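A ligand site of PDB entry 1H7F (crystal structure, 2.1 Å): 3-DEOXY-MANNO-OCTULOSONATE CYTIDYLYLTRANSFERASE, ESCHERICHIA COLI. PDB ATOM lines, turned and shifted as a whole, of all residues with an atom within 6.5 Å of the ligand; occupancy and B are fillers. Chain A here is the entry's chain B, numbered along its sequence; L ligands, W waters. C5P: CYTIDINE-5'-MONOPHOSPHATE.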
ATOM      1  N   ILE A   7     -27.344  21.712 -21.711  1.00  0.00           N
ATOM      2  CA  ILE A   7     -27.126  22.192 -20.354  1.00  0.00           C
ATOM      3  C   ILE A   7     -26.033  21.362 -19.683  1.00  0.00           C
ATOM      4  O   ILE A   7     -26.238  20.178 -19.395  1.00  0.00           O
ATOM      5  CB  ILE A   7     -28.425  22.095 -19.504  1.00  0.00           C
ATOM      6  CG1 ILE A   7     -29.570  22.824 -20.214  1.00  0.00           C
ATOM      7  CG2 ILE A   7     -28.228  22.777 -18.151  1.00  0.00           C
ATOM      8  CD1 ILE A   7     -30.940  22.461 -19.674  1.00  0.00           C
ATOM      9  N   PRO A   8     -24.826  21.944 -19.530  1.00  0.00           N
ATOM     10  CA  PRO A   8     -23.720  21.239 -18.884  1.00  0.00           C
ATOM     11  C   PRO A   8     -24.058  21.167 -17.408  1.00  0.00           C
ATOM     12  O   PRO A   8     -24.484  22.154 -16.815  1.00  0.00           O
ATOM     13  CB  PRO A   8     -22.533  22.177 -19.129  1.00  0.00           C
ATOM     14  CG  PRO A   8     -22.923  22.950 -20.338  1.00  0.00           C
ATOM     15  CD  PRO A   8     -24.374  23.237 -20.052  1.00  0.00           C
ATOM     16  N   ALA A   9     -23.942  19.980 -16.823  1.00  0.00           N
ATOM     17  CA  ALA A   9     -24.256  19.813 -15.417  1.00  0.00           C
ATOM     18  C   ALA A   9     -23.398  18.728 -14.786  1.00  0.00           C
ATOM     19  O   ALA A   9     -23.827  17.582 -14.660  1.00  0.00           O
ATOM     20  CB  ALA A   9     -25.749  19.459 -15.255  1.00  0.00           C
ATOM     21  N   ARG A  10     -22.158  19.069 -14.471  1.00  0.00           N
ATOM     22  CA  ARG A  10     -21.269  18.121 -13.842  1.00  0.00           C
ATOM     23  C   ARG A  10     -21.715  18.026 -12.389  1.00  0.00           C
ATOM     24  O   ARG A  10     -22.295  18.964 -11.844  1.00  0.00           O
ATOM     25  CB  ARG A  10     -19.813  18.601 -13.928  1.00  0.00           C
ATOM     26  CG  ARG A  10     -19.481  19.838 -13.106  1.00  0.00           C
ATOM     27  CD  ARG A  10     -18.043  20.235 -13.310  1.00  0.00           C
ATOM     28  NE  ARG A  10     -17.291  20.405 -12.070  1.00  0.00           N
ATOM     29  CZ  ARG A  10     -16.312  19.595 -11.661  1.00  0.00           C
ATOM     30  NH1 ARG A  10     -15.957  18.556 -12.410  1.00  0.00           N
ATOM     31  NH2 ARG A  10     -15.696  19.830 -10.513  1.00  0.00           N
ATOM     32  N   TYR A  11     -21.485  16.879 -11.769  1.00  0.00           N
ATOM     33  CA  TYR A  11     -21.886  16.667 -10.384  1.00  0.00           C
ATOM     34  C   TYR A  11     -21.060  17.515  -9.412  1.00  0.00           C
ATOM     35  O   TYR A  11     -21.601  18.179  -8.520  1.00  0.00           O
ATOM     36  CB  TYR A  11     -21.739  15.184 -10.060  1.00  0.00           C
ATOM     37  CG  TYR A  11     -22.228  14.799  -8.683  1.00  0.00           C
ATOM     38  CD1 TYR A  11     -23.566  14.471  -8.476  1.00  0.00           C
ATOM     39  CD2 TYR A  11     -21.353  14.773  -7.598  1.00  0.00           C
ATOM     40  CE1 TYR A  11     -24.026  14.121  -7.205  1.00  0.00           C
ATOM     41  CE2 TYR A  11     -21.802  14.428  -6.334  1.00  0.00           C
ATOM     42  CZ  TYR A  11     -23.137  14.112  -6.143  1.00  0.00           C
ATOM     43  OH  TYR A  11     -23.585  13.781  -4.881  1.00  0.00           O
ATOM     44  N   GLY A  12     -19.747  17.537  -9.631  1.00  0.00           N
ATOM     45  CA  GLY A  12     -18.848  18.260  -8.765  1.00  0.00           C
ATOM     46  C   GLY A  12     -18.908  19.765  -8.636  1.00  0.00           C
ATOM     47  O   GLY A  12     -19.333  20.479  -9.552  1.00  0.00           O
ATOM     48  N   SER A  13     -18.425  20.240  -7.500  1.00  0.00           N
ATOM     49  CA  SER A  13     -18.350  21.664  -7.158  1.00  0.00           C
ATOM     50  C   SER A  13     -17.615  21.739  -5.827  1.00  0.00           C
ATOM     51  O   SER A  13     -17.959  21.026  -4.881  1.00  0.00           O
ATOM     52  CB  SER A  13     -19.732  22.281  -7.041  1.00  0.00           C
ATOM     53  OG  SER A  13     -19.642  23.652  -6.671  1.00  0.00           O
ATOM     54  N   LYS A  19     -24.125  19.798  -6.927  1.00  0.00           N
ATOM     55  CA  LYS A  19     -24.892  21.017  -7.187  1.00  0.00           C
ATOM     56  C   LYS A  19     -26.166  20.903  -8.037  1.00  0.00           C
ATOM     57  O   LYS A  19     -27.185  21.487  -7.683  1.00  0.00           O
ATOM     58  CB  LYS A  19     -23.979  22.109  -7.769  1.00  0.00           C
ATOM     59  CG  LYS A  19     -24.607  23.492  -7.751  1.00  0.00           C
ATOM     60  CD  LYS A  19     -23.587  24.620  -7.878  1.00  0.00           C
ATOM     61  CE  LYS A  19     -22.878  24.589  -9.209  1.00  0.00           C
ATOM     62  NZ  LYS A  19     -22.039  25.821  -9.350  1.00  0.00           N
ATOM     63  N   PRO A  20     -26.130  20.176  -9.160  1.00  0.00           N
ATOM     64  CA  PRO A  20     -27.337  20.065  -9.984  1.00  0.00           C
ATOM     65  C   PRO A  20     -28.530  19.364  -9.342  1.00  0.00           C
ATOM     66  O   PRO A  20     -29.667  19.517  -9.799  1.00  0.00           O
ATOM     67  CB  PRO A  20     -26.852  19.307 -11.227  1.00  0.00           C
ATOM     68  CG  PRO A  20     -25.654  18.558 -10.738  1.00  0.00           C
ATOM     69  CD  PRO A  20     -24.976  19.559  -9.850  1.00  0.00           C
ATOM     70  N   ALA A  49     -26.047  17.588 -20.380  1.00  0.00           N
ATOM     71  CA  ALA A  49     -24.781  16.892 -20.582  1.00  0.00           C
ATOM     72  C   ALA A  49     -24.178  16.789 -19.185  1.00  0.00           C
ATOM     73  O   ALA A  49     -23.979  17.795 -18.514  1.00  0.00           O
ATOM     74  CB  ALA A  49     -23.872  17.700 -21.507  1.00  0.00           C
ATOM     75  N   ASN A  71     -15.500  12.922 -17.940  1.00  0.00           N
ATOM     76  CA  ASN A  71     -15.328  13.621 -16.677  1.00  0.00           C
ATOM     77  C   ASN A  71     -14.070  14.479 -16.648  1.00  0.00           C
ATOM     78  O   ASN A  71     -13.842  15.194 -15.679  1.00  0.00           O
ATOM     79  CB  ASN A  71     -15.305  12.635 -15.505  1.00  0.00           C
ATOM     80  CG  ASN A  71     -14.266  11.526 -15.667  1.00  0.00           C
ATOM     81  OD1 ASN A  71     -14.605  10.377 -15.913  1.00  0.00           O
ATOM     82  ND2 ASN A  71     -12.995  11.882 -15.518  1.00  0.00           N
ATOM     83  N   ASP A  72     -13.268  14.436 -17.715  1.00  0.00           N
ATOM     84  CA  ASP A  72     -12.037  15.215 -17.755  1.00  0.00           C
ATOM     85  C   ASP A  72     -12.094  16.581 -18.443  1.00  0.00           C
ATOM     86  O   ASP A  72     -11.063  17.206 -18.656  1.00  0.00           O
ATOM     87  CB  ASP A  72     -10.891  14.375 -18.339  1.00  0.00           C
ATOM     88  CG  ASP A  72     -11.173  13.861 -19.731  1.00  0.00           C
ATOM     89  OD1 ASP A  72     -11.977  14.472 -20.467  1.00  0.00           O
ATOM     90  OD2 ASP A  72     -10.567  12.832 -20.088  1.00  0.00           O
ATOM     91  N   HIS A  73     -13.298  17.053 -18.776  1.00  0.00           N
ATOM     92  CA  HIS A  73     -13.458  18.356 -19.402  1.00  0.00           C
ATOM     93  C   HIS A  73     -13.195  19.452 -18.371  1.00  0.00           C
ATOM     94  O   HIS A  73     -13.603  19.327 -17.221  1.00  0.00           O
ATOM     95  CB  HIS A  73     -14.867  18.528 -19.981  1.00  0.00           C
ATOM     96  CG  HIS A  73     -15.160  17.624 -21.134  1.00  0.00           C
ATOM     97  ND1 HIS A  73     -14.322  17.531 -22.228  1.00  0.00           N
ATOM     98  CD2 HIS A  73     -16.185  16.773 -21.370  1.00  0.00           C
ATOM     99  CE1 HIS A  73     -14.823  16.653 -23.087  1.00  0.00           C
ATOM    100  NE2 HIS A  73     -15.950  16.179 -22.587  1.00  0.00           N
ATOM    101  N   GLU A  74     -12.535  20.520 -18.797  1.00  0.00           N
ATOM    102  CA  GLU A  74     -12.225  21.627 -17.906  1.00  0.00           C
ATOM    103  C   GLU A  74     -13.332  22.647 -17.863  1.00  0.00           C
ATOM    104  O   GLU A  74     -13.439  23.420 -16.904  1.00  0.00           O
ATOM    105  CB  GLU A  74     -10.938  22.311 -18.349  1.00  0.00           C
ATOM    106  CG  GLU A  74      -9.745  21.387 -18.471  1.00  0.00           C
ATOM    107  CD  GLU A  74      -8.593  22.031 -19.218  1.00  0.00           C
ATOM    108  OE1 GLU A  74      -8.823  22.513 -20.347  1.00  0.00           O
ATOM    109  OE2 GLU A  74      -7.466  22.057 -18.670  1.00  0.00           O
ATOM    110  N   SER A  75     -14.153  22.679 -18.910  1.00  0.00           N
ATOM    111  CA  SER A  75     -15.258  23.630 -18.984  1.00  0.00           C
ATOM    112  C   SER A  75     -16.470  23.071 -19.703  1.00  0.00           C
ATOM    113  O   SER A  75     -16.395  22.042 -20.375  1.00  0.00           O
ATOM    114  CB  SER A  75     -14.797  24.899 -19.713  1.00  0.00           C
ATOM    115  OG  SER A  75     -14.404  24.605 -21.031  1.00  0.00           O
ATOM    116  N   GLY A  76     -17.594  23.773 -19.556  1.00  0.00           N
ATOM    117  CA  GLY A  76     -18.822  23.369 -20.202  1.00  0.00           C
ATOM    118  C   GLY A  76     -18.710  23.460 -21.718  1.00  0.00           C
ATOM    119  O   GLY A  76     -19.401  22.733 -22.440  1.00  0.00           O
ATOM    120  N   THR A  77     -17.837  24.345 -22.188  1.00  0.00           N
ATOM    121  CA  THR A  77     -17.611  24.547 -23.611  1.00  0.00           C
ATOM    122  C   THR A  77     -17.030  23.282 -24.201  1.00  0.00           C
ATOM    123  O   THR A  77     -17.506  22.790 -25.214  1.00  0.00           O
ATOM    124  CB  THR A  77     -16.656  25.711 -23.884  1.00  0.00           C
ATOM    125  OG1 THR A  77     -17.162  26.903 -23.256  1.00  0.00           O
ATOM    126  CG2 THR A  77     -16.560  25.953 -25.377  1.00  0.00           C
ATOM    127  N   ARG A  79     -17.257  20.441 -23.008  1.00  0.00           N
ATOM    128  CA  ARG A  79     -18.264  19.399 -22.845  1.00  0.00           C
ATOM    129  C   ARG A  79     -19.247  19.506 -24.006  1.00  0.00           C
ATOM    130  O   ARG A  79     -19.697  18.487 -24.537  1.00  0.00           O
ATOM    131  CB  ARG A  79     -18.997  19.550 -21.501  1.00  0.00           C
ATOM    132  CG  ARG A  79     -19.797  18.312 -21.079  1.00  0.00           C
ATOM    133  CD  ARG A  79     -20.446  18.448 -19.693  1.00  0.00           C
ATOM    134  NE  ARG A  79     -19.467  18.703 -18.635  1.00  0.00           N
ATOM    135  CZ  ARG A  79     -18.579  17.821 -18.169  1.00  0.00           C
ATOM    136  NH1 ARG A  79     -18.524  16.584 -18.666  1.00  0.00           N
ATOM    137  NH2 ARG A  79     -17.707  18.200 -17.254  1.00  0.00           N
ATOM    138  N   ASN A  94     -25.796  27.084 -25.190  1.00  0.00           N
ATOM    139  CA  ASN A  94     -25.208  26.584 -23.960  1.00  0.00           C
ATOM    140  C   ASN A  94     -25.783  27.339 -22.784  1.00  0.00           C
ATOM    141  O   ASN A  94     -25.568  28.535 -22.639  1.00  0.00           O
ATOM    142  CB  ASN A  94     -23.701  26.802 -23.978  1.00  0.00           C
ATOM    143  CG  ASN A  94     -22.947  25.773 -23.173  1.00  0.00           C
ATOM    144  OD1 ASN A  94     -23.222  24.574 -23.271  1.00  0.00           O
ATOM    145  ND2 ASN A  94     -21.981  26.231 -22.383  1.00  0.00           N
ATOM    146  N   LEU A  95     -26.554  26.643 -21.953  1.00  0.00           N
ATOM    147  CA  LEU A  95     -27.160  27.242 -20.764  1.00  0.00           C
ATOM    148  C   LEU A  95     -26.433  26.763 -19.519  1.00  0.00           C
ATOM    149  O   LEU A  95     -26.010  25.611 -19.435  1.00  0.00           O
ATOM    150  CB  LEU A  95     -28.634  26.843 -20.641  1.00  0.00           C
ATOM    151  CG  LEU A  95     -29.660  27.565 -21.503  1.00  0.00           C
ATOM    152  CD1 LEU A  95     -31.061  27.104 -21.116  1.00  0.00           C
ATOM    153  CD2 LEU A  95     -29.541  29.053 -21.293  1.00  0.00           C
ATOM    154  N   GLN A  96     -26.292  27.644 -18.530  1.00  0.00           N
ATOM    155  CA  GLN A  96     -25.638  27.275 -17.286  1.00  0.00           C
ATOM    156  C   GLN A  96     -26.581  26.407 -16.442  1.00  0.00           C
ATOM    157  O   GLN A  96     -27.751  26.752 -16.247  1.00  0.00           O
ATOM    158  CB  GLN A  96     -25.228  28.523 -16.503  1.00  0.00           C
ATOM    159  CG  GLN A  96     -24.261  29.418 -17.252  1.00  0.00           C
ATOM    160  CD  GLN A  96     -23.070  28.638 -17.752  1.00  0.00           C
ATOM    161  OE1 GLN A  96     -22.107  28.419 -17.019  1.00  0.00           O
ATOM    162  NE2 GLN A  96     -23.125  28.198 -19.006  1.00  0.00           N
ATOM    163  N   GLY A  97     -26.075  25.258 -15.990  1.00  0.00           N
ATOM    164  CA  GLY A  97     -26.872  24.365 -15.172  1.00  0.00           C
ATOM    165  C   GLY A  97     -27.179  24.889 -13.784  1.00  0.00           C
ATOM    166  O   GLY A  97     -27.988  24.291 -13.078  1.00  0.00           O
ATOM    167  N   ASP A  98     -26.590  26.023 -13.406  1.00  0.00           N
ATOM    168  CA  ASP A  98     -26.793  26.602 -12.085  1.00  0.00           C
ATOM    169  C   ASP A  98     -27.473  27.951 -12.062  1.00  0.00           C
ATOM    170  O   ASP A  98     -27.276  28.742 -11.145  1.00  0.00           O
ATOM    171  CB  ASP A  98     -25.462  26.660 -11.321  1.00  0.00           C
ATOM    172  CG  ASP A  98     -24.399  27.465 -12.039  1.00  0.00           C
ATOM    173  OD1 ASP A  98     -24.588  27.826 -13.215  1.00  0.00           O
ATOM    174  OD2 ASP A  98     -23.360  27.749 -11.410  1.00  0.00           O
ATOM    175  N   VAL A 224     -26.278  29.899  -8.779  1.00  0.00           N
ATOM    176  CA  VAL A 224     -25.979  29.204  -7.524  1.00  0.00           C
ATOM    177  C   VAL A 224     -24.559  28.651  -7.470  1.00  0.00           C
ATOM    178  O   VAL A 224     -24.284  27.549  -7.949  1.00  0.00           O
ATOM    179  CB  VAL A 224     -27.001  28.072  -7.278  1.00  0.00           C
ATOM    180  CG1 VAL A 224     -26.664  27.322  -6.003  1.00  0.00           C
ATOM    181  CG2 VAL A 224     -28.397  28.647  -7.191  1.00  0.00           C
ATOM    182  N   ASP A 225     -23.663  29.420  -6.865  1.00  0.00           N
ATOM    183  CA  ASP A 225     -22.259  29.043  -6.735  1.00  0.00           C
ATOM    184  C   ASP A 225     -21.898  28.743  -5.282  1.00  0.00           C
ATOM    185  O   ASP A 225     -21.170  27.785  -4.992  1.00  0.00           O
ATOM    186  CB  ASP A 225     -21.362  30.175  -7.233  1.00  0.00           C
ATOM    187  CG  ASP A 225     -21.599  30.506  -8.692  1.00  0.00           C
ATOM    188  OD1 ASP A 225     -21.224  29.701  -9.563  1.00  0.00           O
ATOM    189  OD2 ASP A 225     -22.188  31.585  -8.975  1.00  0.00           O
HETATM  190  O3P C5P L   1     -18.399  24.912 -12.367  1.00  0.00           O
HETATM  191  P   C5P L   1     -19.423  25.996 -12.447  1.00  0.00           P
HETATM  192  O1P C5P L   1     -18.866  27.226 -11.794  1.00  0.00           O
HETATM  193  O2P C5P L   1     -20.755  25.560 -11.670  1.00  0.00           O
HETATM  194  O5' C5P L   1     -19.759  26.323 -13.975  1.00  0.00           O
HETATM  195  C5' C5P L   1     -20.994  26.656 -14.622  1.00  0.00           C
HETATM  196  C4' C5P L   1     -21.532  25.559 -15.596  1.00  0.00           C
HETATM  197  O4' C5P L   1     -20.447  24.919 -16.301  1.00  0.00           O
HETATM  198  C3' C5P L   1     -22.315  24.432 -14.893  1.00  0.00           C
HETATM  199  O3' C5P L   1     -23.474  24.122 -15.693  1.00  0.00           O
HETATM  200  C2' C5P L   1     -21.300  23.276 -14.872  1.00  0.00           C
HETATM  201  O2' C5P L   1     -21.879  21.970 -14.806  1.00  0.00           O
HETATM  202  C1' C5P L   1     -20.524  23.484 -16.191  1.00  0.00           C
HETATM  203  N1  C5P L   1     -19.221  22.822 -16.158  1.00  0.00           N
HETATM  204  C2  C5P L   1     -19.023  21.628 -16.771  1.00  0.00           C
HETATM  205  N3  C5P L   1     -17.721  20.989 -16.736  1.00  0.00           N
HETATM  206  C4  C5P L   1     -16.722  21.516 -16.124  1.00  0.00           C
HETATM  207  C5  C5P L   1     -16.964  22.819 -15.448  1.00  0.00           C
HETATM  208  C6  C5P L   1     -18.173  23.403 -15.490  1.00  0.00           C
HETATM  209  O2  C5P L   1     -19.898  21.038 -17.390  1.00  0.00           O
HETATM  210  N4  C5P L   1     -15.543  20.953 -16.085  1.00  0.00           N
HETATM  211  O   HOH W   1     -22.387  21.666 -11.772  1.00  0.00           O
HETATM  212  O   HOH W   2     -17.733  25.826 -17.899  1.00  0.00           O
HETATM  213  O   HOH W   3     -21.002  28.963 -11.891  1.00  0.00           O
HETATM  214  O   HOH W   4     -20.141  22.821 -10.788  1.00  0.00           O
HETATM  215  O   HOH W   5     -21.696  26.089 -19.293  1.00  0.00           O
HETATM  216  O   HOH W   6     -22.594  29.477 -13.840  1.00  0.00           O
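The side-chain carboxylate (OD2) of Asp 98 sits close to an oxygen (O2P) of the ligand (3.4 Å). Ala 9 touches the ligand (CA to O2', 3.3 Å). N of Ser 75 touches N4 of the ligand (3.6 Å). Gly 76 touches the ligand (N to C2, 3.8 Å). OE1 of Gln 96 touches C5' of the ligand (3.2 Å). Hydrophobic or aromatic side chains within 4 Å of the ligand: Pro 8. Of the 25 residues printed, 12 come within 4 Å of the ligand. The nearest printed residue that does not touch the ligand is Asp 225 (4.1 Å).
NZ of Lys 19 is in salt-bridge range of OD2 of Asp 98, at 3.1 Å. The side-chain amino group (NZ) of Lys 19 is in salt-bridge range of the side-chain carboxylate (OD1) of Asp 225, at 3.97 Å. NZ of Lys 19 sits close to O of Val 224 (3.2 Å). The backbone NH (N) of Lys 19 sits at hydrogen-bond distance from the backbone carbonyl oxygen (O) of Tyr 11 (3.4 Å). NE of Arg 10 sits at hydrogen-bond distance from O of Gly 12, 3.2 Å away. The backbone carbonyl oxygen (O) of Ala 49 lies within hydrogen-bond range of the backbone NH (N) of Ala 9. O of Asp 98 lies within hydrogen-bond range of N of Val 224 (2.8 Å).
O of Pro 8 sits at hydrogen-bond distance from O3' of the ligand, 2.5 Å away. NZ of Lys 19 is in salt-bridge range of O2P of the ligand (2.7 Å). O2 of the ligand sits at hydrogen-bond distance from NE of Arg 79. The backbone carbonyl oxygen (O) of His 73 sits at hydrogen-bond distance from a nitrogen (N4) of the ligand (2.8 Å). The backbone NH (N) of Gly 97 lies within hydrogen-bond range of an oxygen (O3') of the ligand. N of Arg 10 is in hydrogen-bond range of O2' of the ligand, 2.9 Å away. The backbone carbonyl oxygen (O) of Glu 74 sits close to a nitrogen (N4) of the ligand (3.3 Å).
Water W3 lies within hydrogen-bond range of the side-chain carboxylate of Asp 225 (2.5 Å), the side-chain carboxylate of Asp 98 (2.7 Å) and an oxygen (O1P) of the ligand (2.8 Å). Water W4 bridges O of Gly 12 (2.8 Å) and O2P of the ligand (2.9 Å). Water W1 bridges the backbone carbonyl oxygen (O) of Arg 10 and an oxygen (O2') of the ligand. Water W2 bridges N of Gly 76 (2.6 Å) and O4' of the ligand (3.3 Å). Water W6 bridges OD1 of Asp 98 (2.7 Å) and OE1 of Gln 96 (3.4 Å). Water W5 lies within hydrogen-bond range of the side-chain amide nitrogen (NE2) of Gln 96 (2.6 Å), the side-chain amide nitrogen (ND2) of Asn 94 (3.1 Å) and an oxygen (O4') of the ligand (3.4 Å).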
